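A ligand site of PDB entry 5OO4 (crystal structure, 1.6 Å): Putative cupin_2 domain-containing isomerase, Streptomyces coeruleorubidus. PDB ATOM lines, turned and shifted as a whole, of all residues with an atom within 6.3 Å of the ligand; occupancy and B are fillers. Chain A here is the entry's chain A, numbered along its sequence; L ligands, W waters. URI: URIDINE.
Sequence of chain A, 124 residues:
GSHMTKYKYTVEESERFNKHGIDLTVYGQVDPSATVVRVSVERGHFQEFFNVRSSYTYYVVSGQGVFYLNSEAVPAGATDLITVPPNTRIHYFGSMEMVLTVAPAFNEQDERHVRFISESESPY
An oxygen (O3') of the ligand is in hydrogen-bond range of a ring nitrogen (NE2) of His 45, 3.0 Å away. NZ of Lys 19 is in hydrogen-bond range of O2' of the ligand. The side-chain carboxylate of Glu 111 sits at hydrogen-bond distance from an oxygen (O2') of the ligand (2.6 Å). An oxygen (O5') of the ligand is in hydrogen-bond range of the side-chain hydroxyl (OH) of Tyr 92 (2.7 Å). An oxygen (O5') of the ligand lies within hydrogen-bond range of the side-chain hydroxyl of Tyr 58 (2.7 Å).
The backbone NH (N) of Ile 90 sits at hydrogen-bond distance from the backbone carbonyl oxygen (O) of Phe 49, 2.8 Å away. The backbone NH (N) of Leu 24 sits at hydrogen-bond distance from the backbone carbonyl oxygen (O) of Phe 17 (2.9 Å). The backbone NH (N) of Phe 106 is in hydrogen-bond range of the side-chain hydroxyl (OG1) of Thr 35 (3.2 Å). The backbone NH (N) of Leu 100 is in hydrogen-bond range of the backbone carbonyl oxygen (O) of Val 37, at 2.8 Å. The side-chain carboxylate (OE2) of Glu 111 sits at hydrogen-bond distance from the side-chain hydroxyl (OH) of Tyr 56 (2.7 Å). O of Tyr 92 is in hydrogen-bond range of N of His 45, at 2.8 Å. O of Gln 47 is in hydrogen-bond range of ND1 of His 45.
Ile 22 touches the ligand. Leu 24 touches the ligand (CD2 to O4', 3.5 Å). CG1 of Val 37 touches O4 of the ligand, 3.6 Å away. Phe 49 touches the ligand (CZ to O5', 3.8 Å). Leu 100 touches the ligand. CD2 of Phe 106 touches O4 of the ligand, 3.4 Å away. The nearest printed residue that does not touch the ligand is Phe 17 (4.1 Å).
Water W6 lies within hydrogen-bond range of an oxygen (O4) of the ligand (2.6 Å) and the side-chain hydroxyl of Thr 35 (2.8 Å). Water W4 lies within hydrogen-bond range of O3' of the ligand (2.7 Å), OE1 of Glu 111 (2.8 Å) and OE1 of Gln 47 (2.9 Å). Water W5 lies within hydrogen-bond range of the side-chain hydroxyl (OG1) of Thr 35 and an oxygen (O4) of the ligand.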
ATOM      1  N   PHE A  17     -18.200 -22.900  19.166  1.00  0.00           N
ATOM      2  CA  PHE A  17     -17.549 -22.693  17.887  1.00  0.00           C
ATOM      3  C   PHE A  17     -16.728 -21.421  17.905  1.00  0.00           C
ATOM      4  O   PHE A  17     -16.887 -20.577  18.789  1.00  0.00           O
ATOM      5  CB  PHE A  17     -18.596 -22.644  16.775  1.00  0.00           C
ATOM      6  CG  PHE A  17     -19.638 -21.593  16.972  1.00  0.00           C
ATOM      7  CD1 PHE A  17     -20.753 -21.842  17.758  1.00  0.00           C
ATOM      8  CD2 PHE A  17     -19.497 -20.343  16.395  1.00  0.00           C
ATOM      9  CE1 PHE A  17     -21.710 -20.871  17.955  1.00  0.00           C
ATOM     10  CE2 PHE A  17     -20.457 -19.366  16.580  1.00  0.00           C
ATOM     11  CZ  PHE A  17     -21.564 -19.618  17.370  1.00  0.00           C
ATOM     12  N   LYS A  19     -15.556 -17.941  15.841  1.00  0.00           N
ATOM     13  CA  LYS A  19     -16.115 -16.947  14.917  1.00  0.00           C
ATOM     14  C   LYS A  19     -15.198 -15.736  15.000  1.00  0.00           C
ATOM     15  O   LYS A  19     -15.064 -15.164  16.072  1.00  0.00           O
ATOM     16  CB  LYS A  19     -17.529 -16.582  15.413  1.00  0.00           C
ATOM     17  CG  LYS A  19     -18.373 -15.709  14.498  1.00  0.00           C
ATOM     18  CD  LYS A  19     -19.765 -15.514  15.092  1.00  0.00           C
ATOM     19  CE  LYS A  19     -20.651 -14.610  14.239  1.00  0.00           C
ATOM     20  NZ  LYS A  19     -22.048 -14.544  14.734  1.00  0.00           N
ATOM     21  N   HIS A  20     -14.540 -15.353  13.904  1.00  0.00           N
ATOM     22  CA  HIS A  20     -13.743 -14.125  13.861  1.00  0.00           C
ATOM     23  C   HIS A  20     -12.699 -14.005  14.979  1.00  0.00           C
ATOM     24  O   HIS A  20     -12.406 -12.902  15.423  1.00  0.00           O
ATOM     25  CB  HIS A  20     -14.653 -12.886  13.907  1.00  0.00           C
ATOM     26  CG  HIS A  20     -15.765 -12.903  12.915  1.00  0.00           C
ATOM     27  ND1 HIS A  20     -15.543 -13.092  11.557  1.00  0.00           N
ATOM     28  CD2 HIS A  20     -17.100 -12.748  13.054  1.00  0.00           C
ATOM     29  CE1 HIS A  20     -16.701 -13.051  10.919  1.00  0.00           C
ATOM     30  NE2 HIS A  20     -17.659 -12.840  11.805  1.00  0.00           N
ATOM     31  N   ILE A  22     -12.901 -15.369  18.093  1.00  0.00           N
ATOM     32  CA  ILE A  22     -13.434 -15.617  19.435  1.00  0.00           C
ATOM     33  C   ILE A  22     -14.021 -17.013  19.538  1.00  0.00           C
ATOM     34  O   ILE A  22     -14.465 -17.586  18.535  1.00  0.00           O
ATOM     35  CB  ILE A  22     -14.489 -14.573  19.865  1.00  0.00           C
ATOM     36  CG1 ILE A  22     -15.790 -14.704  19.054  1.00  0.00           C
ATOM     37  CG2 ILE A  22     -13.930 -13.159  19.737  1.00  0.00           C
ATOM     38  CD1 ILE A  22     -16.984 -13.990  19.647  1.00  0.00           C
ATOM     39  N   LEU A  24     -17.040 -18.978  21.148  1.00  0.00           N
ATOM     40  CA  LEU A  24     -18.379 -18.759  21.659  1.00  0.00           C
ATOM     41  C   LEU A  24     -18.936 -20.011  22.297  1.00  0.00           C
ATOM     42  O   LEU A  24     -18.739 -21.101  21.796  1.00  0.00           O
ATOM     43  CB  LEU A  24     -19.308 -18.341  20.529  1.00  0.00           C
ATOM     44  CG  LEU A  24     -19.281 -16.864  20.203  1.00  0.00           C
ATOM     45  CD1 LEU A  24     -19.756 -16.657  18.780  1.00  0.00           C
ATOM     46  CD2 LEU A  24     -20.129 -16.098  21.198  1.00  0.00           C
ATOM     47  N   VAL A  26     -22.685 -20.954  23.108  1.00  0.00           N
ATOM     48  CA  VAL A  26     -24.098 -20.580  22.991  1.00  0.00           C
ATOM     49  C   VAL A  26     -24.924 -21.654  23.673  1.00  0.00           C
ATOM     50  O   VAL A  26     -25.038 -22.800  23.193  1.00  0.00           O
ATOM     51  CB  VAL A  26     -24.514 -20.411  21.515  1.00  0.00           C
ATOM     52  CG1 VAL A  26     -25.983 -20.023  21.429  1.00  0.00           C
ATOM     53  CG2 VAL A  26     -23.632 -19.387  20.824  1.00  0.00           C
ATOM     54  N   THR A  35     -30.758 -12.986  25.467  1.00  0.00           N
ATOM     55  CA  THR A  35     -30.031 -14.226  25.498  1.00  0.00           C
ATOM     56  C   THR A  35     -28.611 -13.989  25.948  1.00  0.00           C
ATOM     57  O   THR A  35     -28.020 -12.943  25.684  1.00  0.00           O
ATOM     58  CB  THR A  35     -30.107 -14.935  24.150  1.00  0.00           C
ATOM     59  OG1 THR A  35     -29.687 -14.046  23.120  1.00  0.00           O
ATOM     60  CG2 THR A  35     -31.548 -15.345  23.857  1.00  0.00           C
ATOM     61  N   VAL A  37     -24.636 -15.549  26.470  1.00  0.00           N
ATOM     62  CA  VAL A  37     -23.621 -16.474  25.960  1.00  0.00           C
ATOM     63  C   VAL A  37     -22.275 -16.181  26.627  1.00  0.00           C
ATOM     64  O   VAL A  37     -22.109 -15.126  27.259  1.00  0.00           O
ATOM     65  CB  VAL A  37     -23.450 -16.383  24.417  1.00  0.00           C
ATOM     66  CG1 VAL A  37     -24.762 -16.672  23.711  1.00  0.00           C
ATOM     67  CG2 VAL A  37     -22.919 -15.031  23.985  1.00  0.00           C
ATOM     68  N   VAL A  39     -18.164 -15.655  25.911  1.00  0.00           N
ATOM     69  CA  VAL A  39     -17.198 -15.311  24.883  1.00  0.00           C
ATOM     70  C   VAL A  39     -15.803 -15.435  25.481  1.00  0.00           C
ATOM     71  O   VAL A  39     -15.530 -14.872  26.530  1.00  0.00           O
ATOM     72  CB  VAL A  39     -17.393 -13.864  24.378  1.00  0.00           C
ATOM     73  CG1 VAL A  39     -16.314 -13.497  23.360  1.00  0.00           C
ATOM     74  CG2 VAL A  39     -18.781 -13.672  23.800  1.00  0.00           C
ATOM     75  N   HIS A  45     -11.414  -9.982  18.340  1.00  0.00           N
ATOM     76  CA  HIS A  45     -12.552 -10.231  17.488  1.00  0.00           C
ATOM     77  C   HIS A  45     -12.224  -9.475  16.197  1.00  0.00           C
ATOM     78  O   HIS A  45     -12.386  -8.261  16.117  1.00  0.00           O
ATOM     79  CB  HIS A  45     -13.824  -9.694  18.157  1.00  0.00           C
ATOM     80  CG  HIS A  45     -15.091 -10.013  17.430  1.00  0.00           C
ATOM     81  ND1 HIS A  45     -15.419  -9.470  16.213  1.00  0.00           N
ATOM     82  CD2 HIS A  45     -16.123 -10.808  17.781  1.00  0.00           C
ATOM     83  CE1 HIS A  45     -16.586  -9.940  15.826  1.00  0.00           C
ATOM     84  NE2 HIS A  45     -17.037 -10.761  16.760  1.00  0.00           N
ATOM     85  N   GLN A  47     -13.173  -8.587  13.322  1.00  0.00           N
ATOM     86  CA  GLN A  47     -14.277  -8.190  12.474  1.00  0.00           C
ATOM     87  C   GLN A  47     -14.981  -7.055  13.186  1.00  0.00           C
ATOM     88  O   GLN A  47     -15.069  -7.054  14.427  1.00  0.00           O
ATOM     89  CB  GLN A  47     -15.253  -9.358  12.306  1.00  0.00           C
ATOM     90  CG  GLN A  47     -16.417  -9.032  11.373  1.00  0.00           C
ATOM     91  CD  GLN A  47     -17.789  -9.362  11.935  1.00  0.00           C
ATOM     92  OE1 GLN A  47     -17.984  -9.543  13.140  1.00  0.00           O
ATOM     93  NE2 GLN A  47     -18.771  -9.423  11.052  1.00  0.00           N
ATOM     94  N   PHE A  49     -18.688  -5.133  13.364  1.00  0.00           N
ATOM     95  CA  PHE A  49     -20.080  -5.368  13.051  1.00  0.00           C
ATOM     96  C   PHE A  49     -20.933  -4.443  13.879  1.00  0.00           C
ATOM     97  O   PHE A  49     -20.444  -3.809  14.798  1.00  0.00           O
ATOM     98  CB  PHE A  49     -20.453  -6.822  13.393  1.00  0.00           C
ATOM     99  CG  PHE A  49     -20.426  -7.115  14.871  1.00  0.00           C
ATOM    100  CD1 PHE A  49     -19.236  -7.471  15.512  1.00  0.00           C
ATOM    101  CD2 PHE A  49     -21.594  -7.010  15.631  1.00  0.00           C
ATOM    102  CE1 PHE A  49     -19.216  -7.723  16.872  1.00  0.00           C
ATOM    103  CE2 PHE A  49     -21.569  -7.259  16.984  1.00  0.00           C
ATOM    104  CZ  PHE A  49     -20.383  -7.617  17.609  1.00  0.00           C
ATOM    105  N   TYR A  56     -25.671  -4.938  23.258  1.00  0.00           N
ATOM    106  CA  TYR A  56     -24.694  -5.975  23.627  1.00  0.00           C
ATOM    107  C   TYR A  56     -23.993  -5.527  24.895  1.00  0.00           C
ATOM    108  O   TYR A  56     -23.298  -4.489  24.918  1.00  0.00           O
ATOM    109  CB  TYR A  56     -23.650  -6.177  22.508  1.00  0.00           C
ATOM    110  CG  TYR A  56     -24.088  -6.966  21.287  1.00  0.00           C
ATOM    111  CD1 TYR A  56     -25.367  -6.819  20.740  1.00  0.00           C
ATOM    112  CD2 TYR A  56     -23.209  -7.834  20.644  1.00  0.00           C
ATOM    113  CE1 TYR A  56     -25.743  -7.519  19.613  1.00  0.00           C
ATOM    114  CE2 TYR A  56     -23.574  -8.528  19.501  1.00  0.00           C
ATOM    115  CZ  TYR A  56     -24.846  -8.360  18.980  1.00  0.00           C
ATOM    116  OH  TYR A  56     -25.232  -9.042  17.842  1.00  0.00           O
ATOM    117  N   TYR A  58     -21.304  -6.684  27.706  1.00  0.00           N
ATOM    118  CA  TYR A  58     -20.218  -7.608  28.006  1.00  0.00           C
ATOM    119  C   TYR A  58     -19.783  -7.431  29.451  1.00  0.00           C
ATOM    120  O   TYR A  58     -19.357  -6.333  29.842  1.00  0.00           O
ATOM    121  CB  TYR A  58     -19.007  -7.349  27.109  1.00  0.00           C
ATOM    122  CG  TYR A  58     -19.228  -7.499  25.617  1.00  0.00           C
ATOM    123  CD1 TYR A  58     -19.833  -6.473  24.882  1.00  0.00           C
ATOM    124  CD2 TYR A  58     -18.793  -8.634  24.939  1.00  0.00           C
ATOM    125  CE1 TYR A  58     -20.014  -6.605  23.515  1.00  0.00           C
ATOM    126  CE2 TYR A  58     -18.974  -8.767  23.573  1.00  0.00           C
ATOM    127  CZ  TYR A  58     -19.580  -7.742  22.862  1.00  0.00           C
ATOM    128  OH  TYR A  58     -19.773  -7.841  21.501  1.00  0.00           O
ATOM    129  N   ILE A  90     -18.901  -2.332  16.573  1.00  0.00           N
ATOM    130  CA  ILE A  90     -18.160  -3.040  17.616  1.00  0.00           C
ATOM    131  C   ILE A  90     -17.005  -3.850  17.020  1.00  0.00           C
ATOM    132  O   ILE A  90     -17.195  -4.623  16.081  1.00  0.00           O
ATOM    133  CB  ILE A  90     -19.079  -4.062  18.334  1.00  0.00           C
ATOM    134  CG1 ILE A  90     -20.218  -3.371  19.083  1.00  0.00           C
ATOM    135  CG2 ILE A  90     -18.280  -4.915  19.330  1.00  0.00           C
ATOM    136  CD1 ILE A  90     -21.392  -4.286  19.376  1.00  0.00           C
ATOM    137  N   TYR A  92     -13.179  -5.621  19.153  1.00  0.00           N
ATOM    138  CA  TYR A  92     -12.398  -5.581  20.391  1.00  0.00           C
ATOM    139  C   TYR A  92     -11.159  -6.426  20.263  1.00  0.00           C
ATOM    140  O   TYR A  92     -11.145  -7.407  19.504  1.00  0.00           O
ATOM    141  CB  TYR A  92     -13.230  -6.011  21.603  1.00  0.00           C
ATOM    142  CG  TYR A  92     -14.093  -7.243  21.394  1.00  0.00           C
ATOM    143  CD1 TYR A  92     -15.335  -7.153  20.796  1.00  0.00           C
ATOM    144  CD2 TYR A  92     -13.651  -8.512  21.797  1.00  0.00           C
ATOM    145  CE1 TYR A  92     -16.129  -8.273  20.593  1.00  0.00           C
ATOM    146  CE2 TYR A  92     -14.442  -9.639  21.606  1.00  0.00           C
ATOM    147  CZ  TYR A  92     -15.677  -9.513  21.002  1.00  0.00           C
ATOM    148  OH  TYR A  92     -16.460 -10.626  20.783  1.00  0.00           O
ATOM    149  N   MET A  98     -15.531 -13.442  28.946  1.00  0.00           N
ATOM    150  CA  MET A  98     -16.670 -12.558  29.122  1.00  0.00           C
ATOM    151  C   MET A  98     -17.995 -13.303  29.099  1.00  0.00           C
ATOM    152  O   MET A  98     -18.100 -14.409  28.565  1.00  0.00           O
ATOM    153  CB  MET A  98     -16.687 -11.508  28.002  1.00  0.00           C
ATOM    154  CG  MET A  98     -15.382 -10.721  27.887  1.00  0.00           C
ATOM    155  SD  MET A  98     -15.442  -9.438  26.645  1.00  0.00           S
ATOM    156  CE  MET A  98     -15.567 -10.405  25.152  1.00  0.00           C
ATOM    157  N   LEU A 100     -21.742 -12.363  27.746  1.00  0.00           N
ATOM    158  CA  LEU A 100     -22.395 -11.376  26.883  1.00  0.00           C
ATOM    159  C   LEU A 100     -23.897 -11.548  26.934  1.00  0.00           C
ATOM    160  O   LEU A 100     -24.411 -12.647  26.739  1.00  0.00           O
ATOM    161  CB  LEU A 100     -21.933 -11.587  25.436  1.00  0.00           C
ATOM    162  CG  LEU A 100     -22.745 -10.901  24.348  1.00  0.00           C
ATOM    163  CD1 LEU A 100     -22.692  -9.378  24.484  1.00  0.00           C
ATOM    164  CD2 LEU A 100     -22.268 -11.334  22.969  1.00  0.00           C
ATOM    165  N   VAL A 102     -27.291 -10.239  25.004  1.00  0.00           N
ATOM    166  CA  VAL A 102     -27.857  -9.565  23.847  1.00  0.00           C
ATOM    167  C   VAL A 102     -29.350  -9.383  24.108  1.00  0.00           C
ATOM    168  O   VAL A 102     -30.085 -10.353  24.292  1.00  0.00           O
ATOM    169  CB  VAL A 102     -27.597 -10.370  22.560  1.00  0.00           C
ATOM    170  CG1 VAL A 102     -28.169  -9.632  21.349  1.00  0.00           C
ATOM    171  CG2 VAL A 102     -26.104 -10.588  22.386  1.00  0.00           C
ATOM    172  N   PHE A 106     -30.715 -12.212  20.702  1.00  0.00           N
ATOM    173  CA  PHE A 106     -29.876 -12.268  19.517  1.00  0.00           C
ATOM    174  C   PHE A 106     -30.606 -12.899  18.343  1.00  0.00           C
ATOM    175  O   PHE A 106     -31.190 -13.976  18.470  1.00  0.00           O
ATOM    176  CB  PHE A 106     -28.607 -13.046  19.812  1.00  0.00           C
ATOM    177  CG  PHE A 106     -27.714 -13.218  18.614  1.00  0.00           C
ATOM    178  CD1 PHE A 106     -26.888 -12.179  18.212  1.00  0.00           C
ATOM    179  CD2 PHE A 106     -27.728 -14.386  17.871  1.00  0.00           C
ATOM    180  CE1 PHE A 106     -26.075 -12.317  17.103  1.00  0.00           C
ATOM    181  CE2 PHE A 106     -26.922 -14.520  16.758  1.00  0.00           C
ATOM    182  CZ  PHE A 106     -26.101 -13.501  16.371  1.00  0.00           C
ATOM    183  N   GLU A 111     -27.659  -8.532  12.640  1.00  0.00           N
ATOM    184  CA  GLU A 111     -26.255  -8.149  12.652  1.00  0.00           C
ATOM    185  C   GLU A 111     -25.807  -7.800  11.230  1.00  0.00           C
ATOM    186  O   GLU A 111     -26.290  -8.363  10.243  1.00  0.00           O
ATOM    187  CB  GLU A 111     -25.396  -9.254  13.246  1.00  0.00           C
ATOM    188  CG  GLU A 111     -24.380  -8.737  14.232  1.00  0.00           C
ATOM    189  CD  GLU A 111     -23.508  -9.834  14.786  1.00  0.00           C
ATOM    190  OE1 GLU A 111     -22.745 -10.419  13.992  1.00  0.00           O
ATOM    191  OE2 GLU A 111     -23.590 -10.089  16.012  1.00  0.00           O
HETATM  192  N1  URI L   1     -22.879 -14.121  19.032  1.00  0.00           N
HETATM  193  C2  URI L   1     -23.369 -15.239  18.395  1.00  0.00           C
HETATM  194  N3  URI L   1     -24.501 -15.782  18.966  1.00  0.00           N
HETATM  195  C4  URI L   1     -25.169 -15.325  20.080  1.00  0.00           C
HETATM  196  C5  URI L   1     -24.610 -14.150  20.674  1.00  0.00           C
HETATM  197  C6  URI L   1     -23.505 -13.599  20.139  1.00  0.00           C
HETATM  198  O2  URI L   1     -22.854 -15.722  17.396  1.00  0.00           O
HETATM  199  O4  URI L   1     -26.182 -15.924  20.464  1.00  0.00           O
HETATM  200  C1' URI L   1     -21.683 -13.493  18.477  1.00  0.00           C
HETATM  201  C2' URI L   1     -21.940 -12.179  17.744  1.00  0.00           C
HETATM  202  C3' URI L   1     -20.539 -11.571  17.786  1.00  0.00           C
HETATM  203  C4' URI L   1     -20.021 -12.012  19.164  1.00  0.00           C
HETATM  204  O2' URI L   1     -22.424 -12.404  16.425  1.00  0.00           O
HETATM  205  O3' URI L   1     -19.715 -12.138  16.770  1.00  0.00           O
HETATM  206  O4' URI L   1     -20.831 -13.146  19.548  1.00  0.00           O
HETATM  207  C5' URI L   1     -20.101 -10.984  20.259  1.00  0.00           C
HETATM  208  O5' URI L   1     -19.013 -10.102  20.202  1.00  0.00           O
HETATM  209  O   HOH W   1     -25.395 -18.112  17.632  1.00  0.00           O
HETATM  210  O   HOH W   2     -23.780 -17.680  15.208  1.00  0.00           O
HETATM  211  O   HOH W   3     -28.333 -17.558  19.903  1.00  0.00           O
HETATM  212  O   HOH W   4     -20.069 -11.123  14.296  1.00  0.00           O
HETATM  213  O   HOH W   5     -26.836 -13.888  23.092  1.00  0.00           O
HETATM  214  O   HOH W   6     -28.275 -16.131  21.987  1.00  0.00           O
